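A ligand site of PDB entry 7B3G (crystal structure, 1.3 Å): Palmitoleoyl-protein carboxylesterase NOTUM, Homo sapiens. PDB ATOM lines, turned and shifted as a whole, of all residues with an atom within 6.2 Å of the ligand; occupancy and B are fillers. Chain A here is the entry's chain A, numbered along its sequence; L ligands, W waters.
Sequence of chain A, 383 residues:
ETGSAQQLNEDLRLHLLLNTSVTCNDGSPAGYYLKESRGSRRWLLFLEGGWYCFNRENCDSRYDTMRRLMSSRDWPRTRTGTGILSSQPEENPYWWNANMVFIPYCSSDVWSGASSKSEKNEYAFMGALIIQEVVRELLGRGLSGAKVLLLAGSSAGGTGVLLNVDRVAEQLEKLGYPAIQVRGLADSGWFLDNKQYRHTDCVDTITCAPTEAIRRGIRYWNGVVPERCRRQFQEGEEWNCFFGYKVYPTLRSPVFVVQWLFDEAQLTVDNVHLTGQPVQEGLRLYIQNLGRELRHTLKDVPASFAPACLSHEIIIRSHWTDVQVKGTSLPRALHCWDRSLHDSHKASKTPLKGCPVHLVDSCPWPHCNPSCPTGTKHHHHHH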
ATOM      1  N   GLY A  49      11.576  33.373   5.181  1.00  0.00           N
ATOM      2  CA  GLY A  49      12.522  32.438   5.755  1.00  0.00           C
ATOM      3  C   GLY A  49      12.669  32.612   7.263  1.00  0.00           C
ATOM      4  O   GLY A  49      11.899  33.326   7.916  1.00  0.00           O
ATOM      5  N   GLY A  50      13.677  31.935   7.806  1.00  0.00           N
ATOM      6  CA  GLY A  50      13.942  32.031   9.235  1.00  0.00           C
ATOM      7  C   GLY A  50      14.344  30.725   9.892  1.00  0.00           C
ATOM      8  O   GLY A  50      13.865  30.416  10.995  1.00  0.00           O
ATOM      9  N   TRP A  51      15.210  29.958   9.249  1.00  0.00           N
ATOM     10  CA  TRP A  51      15.781  28.718   9.803  1.00  0.00           C
ATOM     11  C   TRP A  51      14.656  27.706  10.052  1.00  0.00           C
ATOM     12  O   TRP A  51      13.752  27.583   9.211  1.00  0.00           O
ATOM     13  CB  TRP A  51      16.706  28.994  10.978  1.00  0.00           C
ATOM     14  CG  TRP A  51      17.926  29.753  10.570  1.00  0.00           C
ATOM     15  CD1 TRP A  51      18.086  31.107  10.555  1.00  0.00           C
ATOM     16  CD2 TRP A  51      19.153  29.197  10.102  1.00  0.00           C
ATOM     17  NE1 TRP A  51      19.340  31.429  10.103  1.00  0.00           N
ATOM     18  CE2 TRP A  51      20.025  30.265   9.818  1.00  0.00           C
ATOM     19  CE3 TRP A  51      19.614  27.888   9.886  1.00  0.00           C
ATOM     20  CZ2 TRP A  51      21.316  30.074   9.345  1.00  0.00           C
ATOM     21  CZ3 TRP A  51      20.895  27.697   9.416  1.00  0.00           C
ATOM     22  CH2 TRP A  51      21.733  28.796   9.151  1.00  0.00           C
ATOM     23  N   TYR A  52      14.694  26.989  11.168  1.00  0.00           N
ATOM     24  CA  TYR A  52      13.763  25.913  11.468  1.00  0.00           C
ATOM     25  C   TYR A  52      14.049  25.396  12.867  1.00  0.00           C
ATOM     26  O   TYR A  52      14.981  25.874  13.529  1.00  0.00           O
ATOM     27  CB  TYR A  52      13.913  24.768  10.454  1.00  0.00           C
ATOM     28  CG  TYR A  52      15.294  24.142  10.426  1.00  0.00           C
ATOM     29  CD1 TYR A  52      15.567  22.975  11.127  1.00  0.00           C
ATOM     30  CD2 TYR A  52      16.328  24.722   9.699  1.00  0.00           C
ATOM     31  CE1 TYR A  52      16.826  22.401  11.108  1.00  0.00           C
ATOM     32  CE2 TYR A  52      17.585  24.161   9.673  1.00  0.00           C
ATOM     33  CZ  TYR A  52      17.827  22.997  10.373  1.00  0.00           C
ATOM     34  OH  TYR A  52      19.084  22.436  10.347  1.00  0.00           O
ATOM     35  N   TYR A 105       6.314  32.858   7.619  1.00  0.00           N
ATOM     36  CA  TYR A 105       6.880  31.555   7.943  1.00  0.00           C
ATOM     37  C   TYR A 105       6.621  31.296   9.419  1.00  0.00           C
ATOM     38  O   TYR A 105       7.264  31.896  10.280  1.00  0.00           O
ATOM     39  CB  TYR A 105       8.370  31.585   7.633  1.00  0.00           C
ATOM     40  CG  TYR A 105       9.145  30.306   7.885  1.00  0.00           C
ATOM     41  CD1 TYR A 105       8.617  29.069   7.541  1.00  0.00           C
ATOM     42  CD2 TYR A 105      10.418  30.354   8.416  1.00  0.00           C
ATOM     43  CE1 TYR A 105       9.339  27.898   7.750  1.00  0.00           C
ATOM     44  CE2 TYR A 105      11.155  29.199   8.636  1.00  0.00           C
ATOM     45  CZ  TYR A 105      10.609  27.972   8.300  1.00  0.00           C
ATOM     46  OH  TYR A 105      11.335  26.830   8.516  1.00  0.00           O
ATOM     47  N   VAL A 110      10.878  24.491   7.042  1.00  0.00           N
ATOM     48  CA  VAL A 110      11.431  24.778   5.716  1.00  0.00           C
ATOM     49  C   VAL A 110      10.298  24.583   4.703  1.00  0.00           C
ATOM     50  O   VAL A 110      10.516  24.200   3.555  1.00  0.00           O
ATOM     51  CB  VAL A 110      12.683  23.918   5.455  1.00  0.00           C
ATOM     52  CG1 VAL A 110      13.295  24.142   4.062  1.00  0.00           C
ATOM     53  CG2 VAL A 110      13.727  24.147   6.548  1.00  0.00           C
ATOM     54  N   SER A 154      12.832  33.589   0.253  1.00  0.00           N
ATOM     55  CA  SER A 154      14.206  33.849   0.653  1.00  0.00           C
ATOM     56  C   SER A 154      14.607  32.930   1.807  1.00  0.00           C
ATOM     57  O   SER A 154      13.801  32.668   2.713  1.00  0.00           O
ATOM     58  CB  SER A 154      14.411  35.308   1.081  1.00  0.00           C
ATOM     59  OG  SER A 154      14.170  36.195  -0.002  1.00  0.00           O
ATOM     60  N   SER A 155      15.851  32.456   1.764  1.00  0.00           N
ATOM     61  CA  SER A 155      16.439  31.628   2.836  1.00  0.00           C
ATOM     62  C   SER A 155      15.645  30.323   2.938  1.00  0.00           C
ATOM     63  O   SER A 155      15.516  29.630   1.921  1.00  0.00           O
ATOM     64  CB  SER A 155      16.594  32.437   4.111  1.00  0.00           C
ATOM     65  OG  SER A 155      17.405  33.581   3.887  1.00  0.00           O
ATOM     66  N   ALA A 156      15.123  29.963   4.107  1.00  0.00           N
ATOM     67  CA  ALA A 156      14.278  28.769   4.199  1.00  0.00           C
ATOM     68  C   ALA A 156      13.094  28.863   3.254  1.00  0.00           C
ATOM     69  O   ALA A 156      12.594  27.836   2.780  1.00  0.00           O
ATOM     70  CB  ALA A 156      13.809  28.571   5.639  1.00  0.00           C
ATOM     71  N   GLY A 157      12.621  30.086   2.966  1.00  0.00           N
ATOM     72  CA  GLY A 157      11.585  30.255   1.981  1.00  0.00           C
ATOM     73  C   GLY A 157      12.054  29.975   0.562  1.00  0.00           C
ATOM     74  O   GLY A 157      11.265  29.531  -0.278  1.00  0.00           O
ATOM     75  N   THR A 159      14.390  27.660  -0.217  1.00  0.00           N
ATOM     76  CA  THR A 159      14.298  26.201  -0.271  1.00  0.00           C
ATOM     77  C   THR A 159      12.843  25.768  -0.353  1.00  0.00           C
ATOM     78  O   THR A 159      12.511  24.803  -1.060  1.00  0.00           O
ATOM     79  CB  THR A 159      14.977  25.596   0.958  1.00  0.00           C
ATOM     80  OG1 THR A 159      16.304  26.135   1.087  1.00  0.00           O
ATOM     81  CG2 THR A 159      15.077  24.083   0.818  1.00  0.00           C
ATOM     82  N   SER A 188      18.528  32.653  -2.017  1.00  0.00           N
ATOM     83  CA  SER A 188      19.326  32.294  -0.841  1.00  0.00           C
ATOM     84  C   SER A 188      18.877  30.981  -0.204  1.00  0.00           C
ATOM     85  O   SER A 188      18.979  30.801   1.014  1.00  0.00           O
ATOM     86  CB  SER A 188      19.368  33.426   0.184  1.00  0.00           C
ATOM     87  OG  SER A 188      20.000  34.576  -0.359  1.00  0.00           O
ATOM     88  N   GLY A 189      18.375  30.058  -1.018  1.00  0.00           N
ATOM     89  CA  GLY A 189      17.966  28.761  -0.519  1.00  0.00           C
ATOM     90  C   GLY A 189      18.650  27.604  -1.222  1.00  0.00           C
ATOM     91  O   GLY A 189      18.152  26.481  -1.202  1.00  0.00           O
ATOM     92  N   PHE A 191      21.802  25.571  -1.092  1.00  0.00           N
ATOM     93  CA  PHE A 191      22.881  25.264  -0.155  1.00  0.00           C
ATOM     94  C   PHE A 191      23.623  24.010  -0.577  1.00  0.00           C
ATOM     95  O   PHE A 191      23.121  23.178  -1.336  1.00  0.00           O
ATOM     96  CB  PHE A 191      22.317  25.073   1.253  1.00  0.00           C
ATOM     97  CG  PHE A 191      21.694  26.305   1.815  1.00  0.00           C
ATOM     98  CD1 PHE A 191      22.477  27.404   2.150  1.00  0.00           C
ATOM     99  CD2 PHE A 191      20.321  26.395   1.987  1.00  0.00           C
ATOM    100  CE1 PHE A 191      21.905  28.550   2.653  1.00  0.00           C
ATOM    101  CE2 PHE A 191      19.746  27.544   2.481  1.00  0.00           C
ATOM    102  CZ  PHE A 191      20.529  28.611   2.819  1.00  0.00           C
ATOM    103  N   PRO A 210      23.761  20.174   9.153  1.00  0.00           N
ATOM    104  CA  PRO A 210      22.528  20.520   8.448  1.00  0.00           C
ATOM    105  C   PRO A 210      21.839  19.300   7.869  1.00  0.00           C
ATOM    106  O   PRO A 210      20.643  19.140   8.062  1.00  0.00           O
ATOM    107  CB  PRO A 210      23.002  21.431   7.325  1.00  0.00           C
ATOM    108  CG  PRO A 210      24.268  22.014   7.808  1.00  0.00           C
ATOM    109  CD  PRO A 210      24.879  21.076   8.803  1.00  0.00           C
ATOM    110  N   THR A 211      22.592  18.459   7.147  1.00  0.00           N
ATOM    111  CA  THR A 211      22.015  17.208   6.653  1.00  0.00           C
ATOM    112  C   THR A 211      21.393  16.423   7.790  1.00  0.00           C
ATOM    113  O   THR A 211      20.271  15.921   7.670  1.00  0.00           O
ATOM    114  CB  THR A 211      23.056  16.354   5.943  1.00  0.00           C
ATOM    115  OG1 THR A 211      24.064  15.922   6.871  1.00  0.00           O
ATOM    116  CG2 THR A 211      23.694  17.109   4.793  1.00  0.00           C
ATOM    117  N   ALA A 213      20.392  17.463  10.769  1.00  0.00           N
ATOM    118  CA  ALA A 213      19.260  18.191  11.347  1.00  0.00           C
ATOM    119  C   ALA A 213      18.057  18.159  10.419  1.00  0.00           C
ATOM    120  O   ALA A 213      16.918  18.049  10.877  1.00  0.00           O
ATOM    121  CB  ALA A 213      19.676  19.634  11.649  1.00  0.00           C
ATOM    122  N   ILE A 214      18.280  18.253   9.108  1.00  0.00           N
ATOM    123  CA  ILE A 214      17.188  18.072   8.151  1.00  0.00           C
ATOM    124  C   ILE A 214      16.658  16.647   8.203  1.00  0.00           C
ATOM    125  O   ILE A 214      15.448  16.421   8.233  1.00  0.00           O
ATOM    126  CB  ILE A 214      17.607  18.488   6.727  1.00  0.00           C
ATOM    127  CG1 ILE A 214      17.872  19.995   6.662  1.00  0.00           C
ATOM    128  CG2 ILE A 214      16.534  18.099   5.723  1.00  0.00           C
ATOM    129  CD1 ILE A 214      16.708  20.843   7.129  1.00  0.00           C
ATOM    130  N   PHE A 242      16.262  18.612  -0.065  1.00  0.00           N
ATOM    131  CA  PHE A 242      16.351  19.968   0.472  1.00  0.00           C
ATOM    132  C   PHE A 242      17.529  20.747  -0.101  1.00  0.00           C
ATOM    133  O   PHE A 242      17.663  21.938   0.174  1.00  0.00           O
ATOM    134  CB  PHE A 242      16.487  19.922   2.003  1.00  0.00           C
ATOM    135  CG  PHE A 242      15.188  19.692   2.720  1.00  0.00           C
ATOM    136  CD1 PHE A 242      14.459  18.527   2.523  1.00  0.00           C
ATOM    137  CD2 PHE A 242      14.694  20.633   3.610  1.00  0.00           C
ATOM    138  CE1 PHE A 242      13.269  18.316   3.188  1.00  0.00           C
ATOM    139  CE2 PHE A 242      13.506  20.432   4.277  1.00  0.00           C
ATOM    140  CZ  PHE A 242      12.793  19.269   4.065  1.00  0.00           C
ATOM    141  N   PHE A 243      18.369  20.098  -0.900  1.00  0.00           N
ATOM    142  CA  PHE A 243      19.564  20.719  -1.465  1.00  0.00           C
ATOM    143  C   PHE A 243      19.322  21.019  -2.931  1.00  0.00           C
ATOM    144  O   PHE A 243      19.050  20.107  -3.719  1.00  0.00           O
ATOM    145  CB  PHE A 243      20.787  19.854  -1.210  1.00  0.00           C
ATOM    146  CG  PHE A 243      21.189  19.808   0.236  1.00  0.00           C
ATOM    147  CD1 PHE A 243      22.056  20.757   0.745  1.00  0.00           C
ATOM    148  CD2 PHE A 243      20.627  18.882   1.093  1.00  0.00           C
ATOM    149  CE1 PHE A 243      22.401  20.742   2.077  1.00  0.00           C
ATOM    150  CE2 PHE A 243      20.966  18.865   2.437  1.00  0.00           C
ATOM    151  CZ  PHE A 243      21.857  19.806   2.925  1.00  0.00           C
ATOM    152  N   ASP A 263      27.412  32.821   0.513  1.00  0.00           N
ATOM    153  CA  ASP A 263      26.258  33.123   1.358  1.00  0.00           C
ATOM    154  C   ASP A 263      26.644  33.003   2.824  1.00  0.00           C
ATOM    155  O   ASP A 263      27.283  32.032   3.240  1.00  0.00           O
ATOM    156  CB  ASP A 263      25.123  32.154   1.028  1.00  0.00           C
ATOM    157  CG  ASP A 263      23.826  32.515   1.719  1.00  0.00           C
ATOM    158  OD1 ASP A 263      23.598  32.021   2.835  1.00  0.00           O
ATOM    159  OD2 ASP A 263      23.052  33.309   1.140  1.00  0.00           O
ATOM    160  N   ALA A 265      24.865  32.425   5.443  1.00  0.00           N
ATOM    161  CA  ALA A 265      24.282  31.280   6.133  1.00  0.00           C
ATOM    162  C   ALA A 265      25.012  29.993   5.772  1.00  0.00           C
ATOM    163  O   ALA A 265      25.171  29.097   6.609  1.00  0.00           O
ATOM    164  CB  ALA A 265      22.794  31.178   5.820  1.00  0.00           C
ATOM    165  N   GLN A 266      25.444  29.868   4.511  1.00  0.00           N
ATOM    166  CA  GLN A 266      26.266  28.732   4.125  1.00  0.00           C
ATOM    167  C   GLN A 266      27.568  28.711   4.910  1.00  0.00           C
ATOM    168  O   GLN A 266      28.005  27.656   5.392  1.00  0.00           O
ATOM    169  CB  GLN A 266      26.560  28.788   2.619  1.00  0.00           C
ATOM    170  CG  GLN A 266      27.482  27.697   2.115  1.00  0.00           C
ATOM    171  CD  GLN A 266      26.782  26.358   1.995  1.00  0.00           C
ATOM    172  OE1 GLN A 266      25.742  26.238   1.349  1.00  0.00           O
ATOM    173  NE2 GLN A 266      27.369  25.330   2.608  1.00  0.00           N
ATOM    174  N   VAL A 269      26.834  27.598   8.680  1.00  0.00           N
ATOM    175  CA  VAL A 269      26.731  26.144   8.846  1.00  0.00           C
ATOM    176  C   VAL A 269      28.063  25.461   8.582  1.00  0.00           C
ATOM    177  O   VAL A 269      28.286  24.337   9.061  1.00  0.00           O
ATOM    178  CB  VAL A 269      25.579  25.543   8.009  1.00  0.00           C
ATOM    179  CG1 VAL A 269      24.245  26.168   8.399  1.00  0.00           C
ATOM    180  CG2 VAL A 269      25.843  25.700   6.527  1.00  0.00           C
ATOM    181  N   HIS A 312      23.595  37.849   2.283  1.00  0.00           N
ATOM    182  CA  HIS A 312      22.504  36.936   2.621  1.00  0.00           C
ATOM    183  C   HIS A 312      21.194  37.585   2.222  1.00  0.00           C
ATOM    184  O   HIS A 312      20.877  38.684   2.674  1.00  0.00           O
ATOM    185  CB  HIS A 312      22.515  36.643   4.121  1.00  0.00           C
ATOM    186  CG  HIS A 312      21.523  35.609   4.549  1.00  0.00           C
ATOM    187  ND1 HIS A 312      21.442  34.366   3.962  1.00  0.00           N
ATOM    188  CD2 HIS A 312      20.553  35.653   5.498  1.00  0.00           C
ATOM    189  CE1 HIS A 312      20.468  33.678   4.536  1.00  0.00           C
ATOM    190  NE2 HIS A 312      19.918  34.443   5.465  1.00  0.00           N
ATOM    191  N   GLU A 313      20.433  36.894   1.366  1.00  0.00           N
ATOM    192  CA  GLU A 313      19.168  37.377   0.803  1.00  0.00           C
ATOM    193  C   GLU A 313      19.302  38.587  -0.105  1.00  0.00           C
ATOM    194  O   GLU A 313      20.302  39.313  -0.061  1.00  0.00           O
ATOM    195  CB  GLU A 313      18.083  37.595   1.864  1.00  0.00           C
ATOM    196  CG  GLU A 313      17.831  36.410   2.762  1.00  0.00           C
ATOM    197  CD  GLU A 313      16.768  36.688   3.820  1.00  0.00           C
ATOM    198  OE1 GLU A 313      16.092  35.724   4.240  1.00  0.00           O
ATOM    199  OE2 GLU A 313      16.602  37.856   4.209  1.00  0.00           O
HETATM  200  C1  LIG L   1      19.168  23.540   5.316  1.00  0.00           C
HETATM  201  C2  LIG L   1      19.804  22.772   4.359  1.00  0.00           C
HETATM  202  C3  LIG L   1      19.340  22.775   3.051  1.00  0.00           C
HETATM  203  C4  LIG L   1      18.240  23.544   2.700  1.00  0.00           C
HETATM  204  C5  LIG L   1      17.605  24.321   3.660  1.00  0.00           C
HETATM  205  C6  LIG L   1      18.068  24.309   4.966  1.00  0.00           C
HETATM  206  C7  LIG L   1      18.091  26.915   6.278  1.00  0.00           C
HETATM  207  C8  LIG L   1      17.438  30.592   6.769  1.00  0.00           C
HETATM  208  C9  LIG L   1      19.340  29.383   6.374  1.00  0.00           C
HETATM  209  C10 LIG L   1      20.108  28.249   6.146  1.00  0.00           C
HETATM  210  C11 LIG L   1      19.498  26.998   6.095  1.00  0.00           C
HETATM  211  N1  LIG L   1      17.361  28.025   6.499  1.00  0.00           N
HETATM  212  N2  LIG L   1      18.001  29.253   6.546  1.00  0.00           N
HETATM  213  N3  LIG L   1      18.501  31.526   6.725  1.00  0.00           N
HETATM  214  N4  LIG L   1      19.672  30.824   6.487  1.00  0.00           N
HETATM  215  O1  LIG L   1      16.291  30.833   6.939  1.00  0.00           O
HETATM  216  S1  LIG L   1      17.244  25.322   6.218  1.00  0.00           S
HETATM  217 CL1  LIG L   1      19.758  23.545   7.006  1.00  0.00          CL
HETATM  218  O   HOH W   1      17.918  33.857   7.322  1.00  0.00           O
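N of Trp 51 lies within hydrogen-bond range of O1 of the ligand (2.7 Å). The backbone NH of Ala 156 is in hydrogen-bond range of an oxygen (O1) of the ligand, 3.2 Å away. O1 of the ligand sits at hydrogen-bond distance from N of Gly 50 (3.0 Å). N3 of the ligand lies within hydrogen-bond range of NE2 of His 312, 3.5 Å away.
Water W1 lies within hydrogen-bond range of a nitrogen (N3) of the ligand (2.5 Å), a ring nitrogen (NE2) of His 312 (2.8 Å) and the side-chain hydroxyl of Ser 155 (3.5 Å).
Residues that only touch the ligand: Tyr 52 (3.5 Å), Val 110 (3.7 Å), Ser 155 (3.3 Å), Thr 159 (3.4 Å), Phe 191 (3.4 Å), Pro 210 (3.9 Å), Phe 242 (3.0 Å), Phe 243 (3.8 Å) and Ala 265 (3.2 Å). Hydrophobic or aromatic side chains that line the ligand: Trp 51, Tyr 52, Val 110, Ala 156, Phe 191, Pro 210, Phe 243, Ala 265 and His 312. Of the 26 residues printed, 13 come within 4 Å of the ligand. The nearest printed residue that does not touch the ligand is Ile 214 (4.01 Å).
The side-chain hydroxyl (OG) of Ser 155 lies within hydrogen-bond range of a ring nitrogen (NE2) of His 312 (3.1 Å). N of Ala 265 sits at hydrogen-bond distance from OD1 of Asp 263, 2.9 Å away. N of Val 110 sits at hydrogen-bond distance from OH of Tyr 105, at 2.8 Å. OD1 of Asp 263 lies within hydrogen-bond range of ND1 of His 312, 3.4 Å away. The side-chain hydroxyl (OG1) of Thr 159 sits at hydrogen-bond distance from the backbone carbonyl oxygen (O) of Gly 189, at 3.0 Å. The backbone carbonyl oxygen (O) of Trp 51 lies within hydrogen-bond range of the side-chain hydroxyl (OH) of Tyr 105 (2.6 Å). The side-chain hydroxyl (OG) of Ser 155 is in hydrogen-bond range of the side-chain carboxylate (OE1) of Glu 313 (2.5 Å).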
